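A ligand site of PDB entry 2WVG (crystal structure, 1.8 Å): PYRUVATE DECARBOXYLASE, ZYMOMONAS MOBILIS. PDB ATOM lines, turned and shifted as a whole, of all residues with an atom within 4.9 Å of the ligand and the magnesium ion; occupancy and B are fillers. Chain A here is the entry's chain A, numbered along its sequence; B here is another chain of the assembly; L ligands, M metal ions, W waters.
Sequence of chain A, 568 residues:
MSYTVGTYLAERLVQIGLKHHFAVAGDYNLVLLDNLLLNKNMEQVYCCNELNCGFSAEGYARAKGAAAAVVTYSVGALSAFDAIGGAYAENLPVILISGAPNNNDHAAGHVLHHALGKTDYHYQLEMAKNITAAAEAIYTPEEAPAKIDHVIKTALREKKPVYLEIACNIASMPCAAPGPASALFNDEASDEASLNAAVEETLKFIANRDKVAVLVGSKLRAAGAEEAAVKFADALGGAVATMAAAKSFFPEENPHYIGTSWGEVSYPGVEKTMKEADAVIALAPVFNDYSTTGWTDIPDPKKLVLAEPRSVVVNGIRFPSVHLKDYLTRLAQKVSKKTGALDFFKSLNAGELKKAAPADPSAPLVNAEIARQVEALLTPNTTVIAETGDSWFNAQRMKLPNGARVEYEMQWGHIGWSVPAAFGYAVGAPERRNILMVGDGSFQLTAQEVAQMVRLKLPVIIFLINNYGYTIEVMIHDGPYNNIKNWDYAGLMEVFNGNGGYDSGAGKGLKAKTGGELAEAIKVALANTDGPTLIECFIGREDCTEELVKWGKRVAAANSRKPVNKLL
Water W2 lies within hydrogen-bond range of the backbone carbonyl oxygen (O) of Ile 465 (2.8 Å), an oxygen (O1) of the ligand (3.0 Å), the side-chain amide nitrogen (ND2) of Asn 467 (3.5 Å) and the backbone NH (N) of Asp 440 (3.5 Å).
Water W3 lies within hydrogen-bond range of the backbone carbonyl oxygen of Thr 388, an oxygen (O6) of the ligand, the backbone NH of Gly 439 and the side-chain hydroxyl of Ser 442.
Water W4 lies within hydrogen-bond range of an oxygen (O1) of the ligand (2.7 Å), the side-chain hydroxyl of Ser 391 (2.8 Å) and the backbone NH of Asp 390 (3.4 Å).
OD2 of Asp 440 is in hydrogen-bond range of N of Tyr 468.
The backbone NH (N) of Asp 440 lies within hydrogen-bond range of the backbone carbonyl oxygen (O) of Ile 465.
The side-chain amide nitrogen (ND2) of Asn 467 lies within hydrogen-bond range of the side-chain hydroxyl (OG1) of Thr 471 (3.0 Å).
The side-chain carboxylate (OE1) of Glu 473 lies within hydrogen-bond range of the backbone NH (N) of Asp 27 of chain B (3.5 Å).
Three residues have an atom within 4 Å of the magnesium ion: Asp 440, Asn 467 and Gly 469.
The nearest printed residue that does not touch the magnesium ion is Gly 441 (4.2 Å).
O1 of the ligand is in hydrogen-bond range of N of Asp 390, 3.1 Å away.
O5 of the ligand lies close to N of Gly 441 (2.7 Å).
A nitrogen (N5) of the ligand is in hydrogen-bond range of the backbone NH of Ile 415, at 3.1 Å.
An oxygen (O6) of the ligand is in hydrogen-bond range of the side-chain hydroxyl (OG) of Ser 442 (2.7 Å).
An oxygen (O2) of the ligand lies within hydrogen-bond range of the backbone NH of Thr 471.
A nitrogen (N4) of the ligand is in hydrogen-bond range of the side-chain carboxylate of Glu 50 of chain B, 2.7 Å away.
N of Ile 472 lies within hydrogen-bond range of O2 of the ligand (2.6 Å).
N of Ser 442 is in hydrogen-bond range of O6 of the ligand, at 2.9 Å.
O of Gly 413 sits at hydrogen-bond distance from N6 of the ligand (2.8 Å).
O5 of the ligand lies close to N of Asp 440 (3.5 Å).
The magnesium ion is bound by an oxygen (O5) of the ligand (2.2 Å), the backbone carbonyl oxygen (O) of Gly 469 (2.2 Å), the side-chain amide oxygen (OD1) of Asn 467 (2.2 Å), the side-chain carboxylate (OD1) of Asp 440 (2.2 Å), an oxygen (O3) of the ligand (2.3 Å) and water W2 (2.4 Å).
The magnesium ion has six donor atoms within binding distance.
OE1 of Glu 473 lies close to N3 of the ligand (3.5 Å).
Residues that only touch the ligand: Ala 25 of chain B, His 414, Tyr 470, Gly 439, His 114 of chain B, Gly 389, Gly 26 of chain B, Val 75 of chain B and Thr 388.
Hydrophobic or aromatic side chains that line the ligand: His 414, Ile 415, Tyr 470, Ile 472, Val 75 of chain B and His 114 of chain B.
Of the 29 residues printed, 21 come within 4 Å of the ligand.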
ATOM      1  N   THR A 388       0.209  14.378  12.345  1.00  0.00           N
ATOM      2  CA  THR A 388      -1.131  14.004  12.768  1.00  0.00           C
ATOM      3  C   THR A 388      -2.007  15.250  12.828  1.00  0.00           C
ATOM      4  O   THR A 388      -1.621  16.262  13.424  1.00  0.00           O
ATOM      5  CB  THR A 388      -1.117  13.370  14.163  1.00  0.00           C
ATOM      6  OG1 THR A 388      -0.437  12.111  14.103  1.00  0.00           O
ATOM      7  CG2 THR A 388      -2.529  13.133  14.666  1.00  0.00           C
ATOM      8  N   GLY A 389      -3.175  15.180  12.203  1.00  0.00           N
ATOM      9  CA  GLY A 389      -4.029  16.340  12.055  1.00  0.00           C
ATOM     10  C   GLY A 389      -4.611  16.331  10.650  1.00  0.00           C
ATOM     11  O   GLY A 389      -4.530  15.309   9.959  1.00  0.00           O
ATOM     12  N   ASP A 390      -5.207  17.433  10.218  1.00  0.00           N
ATOM     13  CA  ASP A 390      -5.694  17.463   8.839  1.00  0.00           C
ATOM     14  C   ASP A 390      -4.562  17.299   7.815  1.00  0.00           C
ATOM     15  O   ASP A 390      -4.808  16.910   6.673  1.00  0.00           O
ATOM     16  CB  ASP A 390      -6.511  18.730   8.549  1.00  0.00           C
ATOM     17  CG  ASP A 390      -7.421  18.556   7.345  1.00  0.00           C
ATOM     18  OD1 ASP A 390      -7.868  17.416   7.105  1.00  0.00           O
ATOM     19  OD2 ASP A 390      -7.678  19.554   6.632  1.00  0.00           O
ATOM     20  N   SER A 391      -3.328  17.585   8.229  1.00  0.00           N
ATOM     21  CA  SER A 391      -2.177  17.369   7.351  1.00  0.00           C
ATOM     22  C   SER A 391      -2.075  15.934   6.851  1.00  0.00           C
ATOM     23  O   SER A 391      -1.589  15.694   5.745  1.00  0.00           O
ATOM     24  CB  SER A 391      -0.875  17.810   8.027  1.00  0.00           C
ATOM     25  OG  SER A 391      -0.829  19.225   8.159  1.00  0.00           O
ATOM     26  N   GLY A 413       1.185   8.128  16.378  1.00  0.00           N
ATOM     27  CA  GLY A 413       0.354   9.319  16.271  1.00  0.00           C
ATOM     28  C   GLY A 413       0.525  10.353  17.368  1.00  0.00           C
ATOM     29  O   GLY A 413      -0.447  10.901  17.862  1.00  0.00           O
ATOM     30  N   HIS A 414       1.771  10.618  17.732  1.00  0.00           N
ATOM     31  CA  HIS A 414       2.104  11.583  18.773  1.00  0.00           C
ATOM     32  C   HIS A 414       2.211  12.969  18.155  1.00  0.00           C
ATOM     33  O   HIS A 414       3.154  13.238  17.408  1.00  0.00           O
ATOM     34  CB  HIS A 414       3.451  11.187  19.386  1.00  0.00           C
ATOM     35  CG  HIS A 414       3.855  11.999  20.583  1.00  0.00           C
ATOM     36  ND1 HIS A 414       4.061  13.357  20.535  1.00  0.00           N
ATOM     37  CD2 HIS A 414       4.122  11.624  21.853  1.00  0.00           C
ATOM     38  CE1 HIS A 414       4.412  13.800  21.724  1.00  0.00           C
ATOM     39  NE2 HIS A 414       4.462  12.768  22.548  1.00  0.00           N
ATOM     40  N   ILE A 415       1.268  13.871  18.439  1.00  0.00           N
ATOM     41  CA  ILE A 415       1.366  15.200  17.831  1.00  0.00           C
ATOM     42  C   ILE A 415       2.664  15.849  18.281  1.00  0.00           C
ATOM     43  O   ILE A 415       3.085  15.658  19.421  1.00  0.00           O
ATOM     44  CB  ILE A 415       0.134  16.121  18.094  1.00  0.00           C
ATOM     45  CG1 ILE A 415      -0.079  16.362  19.584  1.00  0.00           C
ATOM     46  CG2 ILE A 415      -1.115  15.579  17.399  1.00  0.00           C
ATOM     47  CD1 ILE A 415      -1.083  17.485  19.849  1.00  0.00           C
ATOM     48  N   GLY A 439       0.478  21.258  11.842  1.00  0.00           N
ATOM     49  CA  GLY A 439      -0.573  22.105  12.395  1.00  0.00           C
ATOM     50  C   GLY A 439      -0.091  22.945  13.556  1.00  0.00           C
ATOM     51  O   GLY A 439       0.891  22.598  14.216  1.00  0.00           O
ATOM     52  N   ASP A 440      -0.794  24.043  13.840  1.00  0.00           N
ATOM     53  CA  ASP A 440      -0.415  24.921  14.951  1.00  0.00           C
ATOM     54  C   ASP A 440      -0.427  24.185  16.302  1.00  0.00           C
ATOM     55  O   ASP A 440       0.445  24.392  17.152  1.00  0.00           O
ATOM     56  CB  ASP A 440      -1.302  26.181  15.008  1.00  0.00           C
ATOM     57  CG  ASP A 440      -2.795  25.856  15.136  1.00  0.00           C
ATOM     58  OD1 ASP A 440      -3.269  24.885  14.528  1.00  0.00           O
ATOM     59  OD2 ASP A 440      -3.508  26.599  15.845  1.00  0.00           O
ATOM     60  N   GLY A 441      -1.411  23.318  16.509  1.00  0.00           N
ATOM     61  CA  GLY A 441      -1.515  22.591  17.768  1.00  0.00           C
ATOM     62  C   GLY A 441      -0.328  21.682  18.016  1.00  0.00           C
ATOM     63  O   GLY A 441       0.246  21.670  19.111  1.00  0.00           O
ATOM     64  N   SER A 442       0.041  20.912  16.993  1.00  0.00           N
ATOM     65  CA  SER A 442       1.185  20.002  17.062  1.00  0.00           C
ATOM     66  C   SER A 442       2.499  20.760  17.214  1.00  0.00           C
ATOM     67  O   SER A 442       3.381  20.362  17.968  1.00  0.00           O
ATOM     68  CB  SER A 442       1.260  19.139  15.805  1.00  0.00           C
ATOM     69  OG  SER A 442       0.123  18.314  15.664  1.00  0.00           O
ATOM     70  N   LEU A 445       3.979  21.607  20.702  1.00  0.00           N
ATOM     71  CA  LEU A 445       4.526  20.607  21.607  1.00  0.00           C
ATOM     72  C   LEU A 445       6.041  20.508  21.538  1.00  0.00           C
ATOM     73  O   LEU A 445       6.689  20.154  22.524  1.00  0.00           O
ATOM     74  CB  LEU A 445       3.929  19.217  21.350  1.00  0.00           C
ATOM     75  CG  LEU A 445       2.572  18.910  21.974  1.00  0.00           C
ATOM     76  CD1 LEU A 445       1.472  19.388  21.045  1.00  0.00           C
ATOM     77  CD2 LEU A 445       2.418  17.420  22.270  1.00  0.00           C
ATOM     78  N   ILE A 465       0.239  25.320   9.456  1.00  0.00           N
ATOM     79  CA  ILE A 465      -1.157  25.581   9.149  1.00  0.00           C
ATOM     80  C   ILE A 465      -1.857  26.121  10.395  1.00  0.00           C
ATOM     81  O   ILE A 465      -2.186  25.379  11.312  1.00  0.00           O
ATOM     82  CB  ILE A 465      -1.872  24.302   8.677  1.00  0.00           C
ATOM     83  CG1 ILE A 465      -1.011  23.555   7.647  1.00  0.00           C
ATOM     84  CG2 ILE A 465      -3.238  24.639   8.100  1.00  0.00           C
ATOM     85  CD1 ILE A 465      -0.689  24.362   6.421  1.00  0.00           C
ATOM     86  N   ASN A 467      -4.929  27.273  11.944  1.00  0.00           N
ATOM     87  CA  ASN A 467      -6.388  27.370  11.983  1.00  0.00           C
ATOM     88  C   ASN A 467      -6.884  27.537  13.413  1.00  0.00           C
ATOM     89  O   ASN A 467      -8.045  27.272  13.722  1.00  0.00           O
ATOM     90  CB  ASN A 467      -7.038  26.158  11.316  1.00  0.00           C
ATOM     91  CG  ASN A 467      -6.609  24.836  11.940  1.00  0.00           C
ATOM     92  OD1 ASN A 467      -6.028  24.831  13.015  1.00  0.00           O
ATOM     93  ND2 ASN A 467      -6.897  23.726  11.268  1.00  0.00           N
ATOM     94  N   TYR A 468      -5.970  27.962  14.286  1.00  0.00           N
ATOM     95  CA  TYR A 468      -6.314  28.364  15.656  1.00  0.00           C
ATOM     96  C   TYR A 468      -6.994  27.249  16.469  1.00  0.00           C
ATOM     97  O   TYR A 468      -8.122  27.410  16.948  1.00  0.00           O
ATOM     98  CB  TYR A 468      -7.160  29.640  15.638  1.00  0.00           C
ATOM     99  CG  TYR A 468      -7.329  30.331  16.981  1.00  0.00           C
ATOM    100  CD1 TYR A 468      -6.311  30.334  17.926  1.00  0.00           C
ATOM    101  CD2 TYR A 468      -8.507  30.988  17.291  1.00  0.00           C
ATOM    102  CE1 TYR A 468      -6.470  30.974  19.157  1.00  0.00           C
ATOM    103  CE2 TYR A 468      -8.680  31.640  18.501  1.00  0.00           C
ATOM    104  CZ  TYR A 468      -7.664  31.629  19.429  1.00  0.00           C
ATOM    105  OH  TYR A 468      -7.854  32.265  20.632  1.00  0.00           O
ATOM    106  N   GLY A 469      -6.317  26.113  16.619  1.00  0.00           N
ATOM    107  CA  GLY A 469      -6.828  25.045  17.459  1.00  0.00           C
ATOM    108  C   GLY A 469      -6.702  23.639  16.893  1.00  0.00           C
ATOM    109  O   GLY A 469      -6.099  23.441  15.837  1.00  0.00           O
ATOM    110  N   TYR A 470      -7.293  22.680  17.586  1.00  0.00           N
ATOM    111  CA  TYR A 470      -7.150  21.252  17.242  1.00  0.00           C
ATOM    112  C   TYR A 470      -8.261  20.749  16.314  1.00  0.00           C
ATOM    113  O   TYR A 470      -9.225  20.138  16.790  1.00  0.00           O
ATOM    114  CB  TYR A 470      -7.209  20.395  18.508  1.00  0.00           C
ATOM    115  CG  TYR A 470      -6.135  20.620  19.544  1.00  0.00           C
ATOM    116  CD1 TYR A 470      -4.870  21.073  19.199  1.00  0.00           C
ATOM    117  CD2 TYR A 470      -6.385  20.313  20.881  1.00  0.00           C
ATOM    118  CE1 TYR A 470      -3.893  21.250  20.169  1.00  0.00           C
ATOM    119  CE2 TYR A 470      -5.424  20.460  21.844  1.00  0.00           C
ATOM    120  CZ  TYR A 470      -4.186  20.939  21.504  1.00  0.00           C
ATOM    121  OH  TYR A 470      -3.238  21.078  22.500  1.00  0.00           O
ATOM    122  N   THR A 471      -8.139  20.965  15.020  1.00  0.00           N
ATOM    123  CA  THR A 471      -9.247  20.647  14.113  1.00  0.00           C
ATOM    124  C   THR A 471      -9.564  19.140  14.026  1.00  0.00           C
ATOM    125  O   THR A 471     -10.725  18.755  13.979  1.00  0.00           O
ATOM    126  CB  THR A 471      -9.030  21.283  12.716  1.00  0.00           C
ATOM    127  OG1 THR A 471      -9.175  22.700  12.837  1.00  0.00           O
ATOM    128  CG2 THR A 471     -10.039  20.761  11.708  1.00  0.00           C
ATOM    129  N   ILE A 472      -8.554  18.293  14.032  1.00  0.00           N
ATOM    130  CA  ILE A 472      -8.864  16.873  13.980  1.00  0.00           C
ATOM    131  C   ILE A 472      -9.681  16.398  15.205  1.00  0.00           C
ATOM    132  O   ILE A 472     -10.504  15.556  15.051  1.00  0.00           O
ATOM    133  CB  ILE A 472      -7.609  15.983  13.758  1.00  0.00           C
ATOM    134  CG1 ILE A 472      -8.005  14.549  13.424  1.00  0.00           C
ATOM    135  CG2 ILE A 472      -6.688  16.206  14.821  1.00  0.00           C
ATOM    136  CD1 ILE A 472      -6.863  13.596  13.099  1.00  0.00           C
ATOM    137  N   GLU A 473      -9.410  16.968  16.370  1.00  0.00           N
ATOM    138  CA  GLU A 473     -10.211  16.636  17.544  1.00  0.00           C
ATOM    139  C   GLU A 473     -11.609  17.242  17.460  1.00  0.00           C
ATOM    140  O   GLU A 473     -12.584  16.629  17.884  1.00  0.00           O
ATOM    141  CB  GLU A 473      -9.503  17.118  18.807  1.00  0.00           C
ATOM    142  CG  GLU A 473      -8.111  16.556  18.997  1.00  0.00           C
ATOM    143  CD  GLU A 473      -8.129  15.059  19.282  1.00  0.00           C
ATOM    144  OE1 GLU A 473      -7.718  14.668  20.398  1.00  0.00           O
ATOM    145  OE2 GLU A 473      -8.551  14.280  18.400  1.00  0.00           O
ATOM    146  N   VAL B  24      -4.413  17.576  28.809  1.00  0.00           N
ATOM    147  CA  VAL B  24      -4.192  17.657  27.369  1.00  0.00           C
ATOM    148  C   VAL B  24      -5.158  16.697  26.683  1.00  0.00           C
ATOM    149  O   VAL B  24      -5.159  15.500  26.952  1.00  0.00           O
ATOM    150  CB  VAL B  24      -2.753  17.288  26.985  1.00  0.00           C
ATOM    151  CG1 VAL B  24      -2.579  17.449  25.481  1.00  0.00           C
ATOM    152  CG2 VAL B  24      -1.758  18.167  27.727  1.00  0.00           C
ATOM    153  N   ALA B  25      -5.994  17.239  25.783  1.00  0.00           N
ATOM    154  CA  ALA B  25      -7.004  16.439  25.106  1.00  0.00           C
ATOM    155  C   ALA B  25      -6.429  15.365  24.193  1.00  0.00           C
ATOM    156  O   ALA B  25      -5.389  15.561  23.547  1.00  0.00           O
ATOM    157  CB  ALA B  25      -7.913  17.345  24.307  1.00  0.00           C
ATOM    158  N   GLY B  26      -7.117  14.225  24.134  1.00  0.00           N
ATOM    159  CA  GLY B  26      -6.835  13.177  23.160  1.00  0.00           C
ATOM    160  C   GLY B  26      -8.100  12.338  23.042  1.00  0.00           C
ATOM    161  O   GLY B  26      -8.910  12.349  23.967  1.00  0.00           O
ATOM    162  N   ASP B  27      -8.285  11.616  21.947  1.00  0.00           N
ATOM    163  CA  ASP B  27      -9.580  10.950  21.751  1.00  0.00           C
ATOM    164  C   ASP B  27      -9.954   9.929  22.850  1.00  0.00           C
ATOM    165  O   ASP B  27     -11.140   9.711  23.126  1.00  0.00           O
ATOM    166  CB  ASP B  27      -9.783  10.419  20.316  1.00  0.00           C
ATOM    167  CG  ASP B  27      -8.823   9.296  19.948  1.00  0.00           C
ATOM    168  OD1 ASP B  27      -7.826   9.058  20.671  1.00  0.00           O
ATOM    169  OD2 ASP B  27      -9.083   8.645  18.908  1.00  0.00           O
ATOM    170  N   GLU B  50       2.348  17.004  27.398  1.00  0.00           N
ATOM    171  CA  GLU B  50       2.054  16.207  28.582  1.00  0.00           C
ATOM    172  C   GLU B  50       3.140  16.241  29.641  1.00  0.00           C
ATOM    173  O   GLU B  50       2.853  16.141  30.830  1.00  0.00           O
ATOM    174  CB  GLU B  50       1.713  14.756  28.202  1.00  0.00           C
ATOM    175  CG  GLU B  50       0.367  14.588  27.506  1.00  0.00           C
ATOM    176  CD  GLU B  50       0.410  14.841  26.002  1.00  0.00           C
ATOM    177  OE1 GLU B  50       1.474  15.220  25.456  1.00  0.00           O
ATOM    178  OE2 GLU B  50      -0.637  14.649  25.355  1.00  0.00           O
ATOM    179  N   THR B  72      -3.873  11.436  27.546  1.00  0.00           N
ATOM    180  CA  THR B  72      -4.381  10.365  26.713  1.00  0.00           C
ATOM    181  C   THR B  72      -3.474   9.123  26.758  1.00  0.00           C
ATOM    182  O   THR B  72      -2.302   9.203  27.140  1.00  0.00           O
ATOM    183  CB  THR B  72      -4.601  10.833  25.257  1.00  0.00           C
ATOM    184  OG1 THR B  72      -5.495   9.917  24.596  1.00  0.00           O
ATOM    185  CG2 THR B  72      -3.284  10.907  24.503  1.00  0.00           C
ATOM    186  N   VAL B  75       0.732   7.821  24.125  1.00  0.00           N
ATOM    187  CA  VAL B  75       1.442   9.018  23.680  1.00  0.00           C
ATOM    188  C   VAL B  75       1.401  10.135  24.713  1.00  0.00           C
ATOM    189  O   VAL B  75       2.329  10.938  24.810  1.00  0.00           O
ATOM    190  CB  VAL B  75       0.901   9.540  22.321  1.00  0.00           C
ATOM    191  CG1 VAL B  75       1.236   8.565  21.201  1.00  0.00           C
ATOM    192  CG2 VAL B  75      -0.597   9.797  22.385  1.00  0.00           C
ATOM    193  N   GLY B  76       0.332  10.216  25.484  1.00  0.00           N
ATOM    194  CA  GLY B  76       0.270  11.203  26.550  1.00  0.00           C
ATOM    195  C   GLY B  76       0.936  10.728  27.833  1.00  0.00           C
ATOM    196  O   GLY B  76       1.765  11.424  28.447  1.00  0.00           O
ATOM    197  N   HIS B 114      -2.139   4.748  18.872  1.00  0.00           N
ATOM    198  CA  HIS B 114      -1.402   5.231  20.041  1.00  0.00           C
ATOM    199  C   HIS B 114      -0.678   4.112  20.794  1.00  0.00           C
ATOM    200  O   HIS B 114       0.017   4.367  21.763  1.00  0.00           O
ATOM    201  CB  HIS B 114      -2.284   5.997  21.039  1.00  0.00           C
ATOM    202  CG  HIS B 114      -2.787   7.314  20.537  1.00  0.00           C
ATOM    203  ND1 HIS B 114      -2.201   7.974  19.473  1.00  0.00           N
ATOM    204  CD2 HIS B 114      -3.792   8.106  20.969  1.00  0.00           C
ATOM    205  CE1 HIS B 114      -2.850   9.111  19.258  1.00  0.00           C
ATOM    206  NE2 HIS B 114      -3.812   9.212  20.159  1.00  0.00           N
HETATM  207  O1  LIG L   1      -4.778  20.371  11.257  1.00  0.00           O
HETATM  208  P1  LIG L   1      -5.203  20.171  12.823  1.00  0.00           P
HETATM  209  O2  LIG L   1      -6.291  18.957  12.955  1.00  0.00           O
HETATM  210  O3  LIG L   1      -5.779  21.401  13.364  1.00  0.00           O
HETATM  211  O4  LIG L   1      -3.817  19.755  13.606  1.00  0.00           O
HETATM  212  P2  LIG L   1      -3.169  20.459  14.926  1.00  0.00           P
HETATM  213  O5  LIG L   1      -3.341  22.066  15.110  1.00  0.00           O
HETATM  214  O6  LIG L   1      -1.737  20.117  14.886  1.00  0.00           O
HETATM  215  O7  LIG L   1      -3.904  19.774  16.219  1.00  0.00           O
HETATM  216  C1  LIG L   1      -3.883  18.378  16.384  1.00  0.00           C
HETATM  217  C2  LIG L   1      -4.783  17.943  17.536  1.00  0.00           C
HETATM  218  C3  LIG L   1      -4.587  16.530  18.067  1.00  0.00           C
HETATM  219  C4  LIG L   1      -4.547  16.182  19.373  1.00  0.00           C
HETATM  220  C5  LIG L   1      -4.632  17.106  20.589  1.00  0.00           C
HETATM  221  N1  LIG L   1      -4.462  15.369  17.284  1.00  0.00           N
HETATM  222  N2  LIG L   1      -4.349  14.345  18.135  1.00  0.00           N
HETATM  223  N3  LIG L   1      -4.387  14.820  19.436  1.00  0.00           N
HETATM  224  C6  LIG L   1      -4.327  14.018  20.663  1.00  0.00           C
HETATM  225  C7  LIG L   1      -2.892  13.872  21.181  1.00  0.00           C
HETATM  226  C8  LIG L   1      -2.544  14.400  22.355  1.00  0.00           C
HETATM  227  N4  LIG L   1      -1.272  14.306  22.805  1.00  0.00           N
HETATM  228  C9  LIG L   1      -0.307  13.646  22.022  1.00  0.00           C
HETATM  229  C10 LIG L   1       1.137  13.593  22.492  1.00  0.00           C
HETATM  230  N5  LIG L   1      -0.654  13.110  20.794  1.00  0.00           N
HETATM  231  C11 LIG L   1      -1.884  13.194  20.376  1.00  0.00           C
HETATM  232  N6  LIG L   1      -2.252  12.591  19.115  1.00  0.00           N
HETATM  233 MG    MG M   1      -4.787  23.317  14.069  1.00  0.00          MG
HETATM  234  O   HOH W   1      -4.990  11.200  17.470  1.00  0.00           O
HETATM  235  O   HOH W   2      -3.591  23.054  11.996  1.00  0.00           O
HETATM  236  O   HOH W   3      -0.873  18.716  12.712  1.00  0.00           O
HETATM  237  O   HOH W   4      -2.370  19.356  10.437  1.00  0.00           O
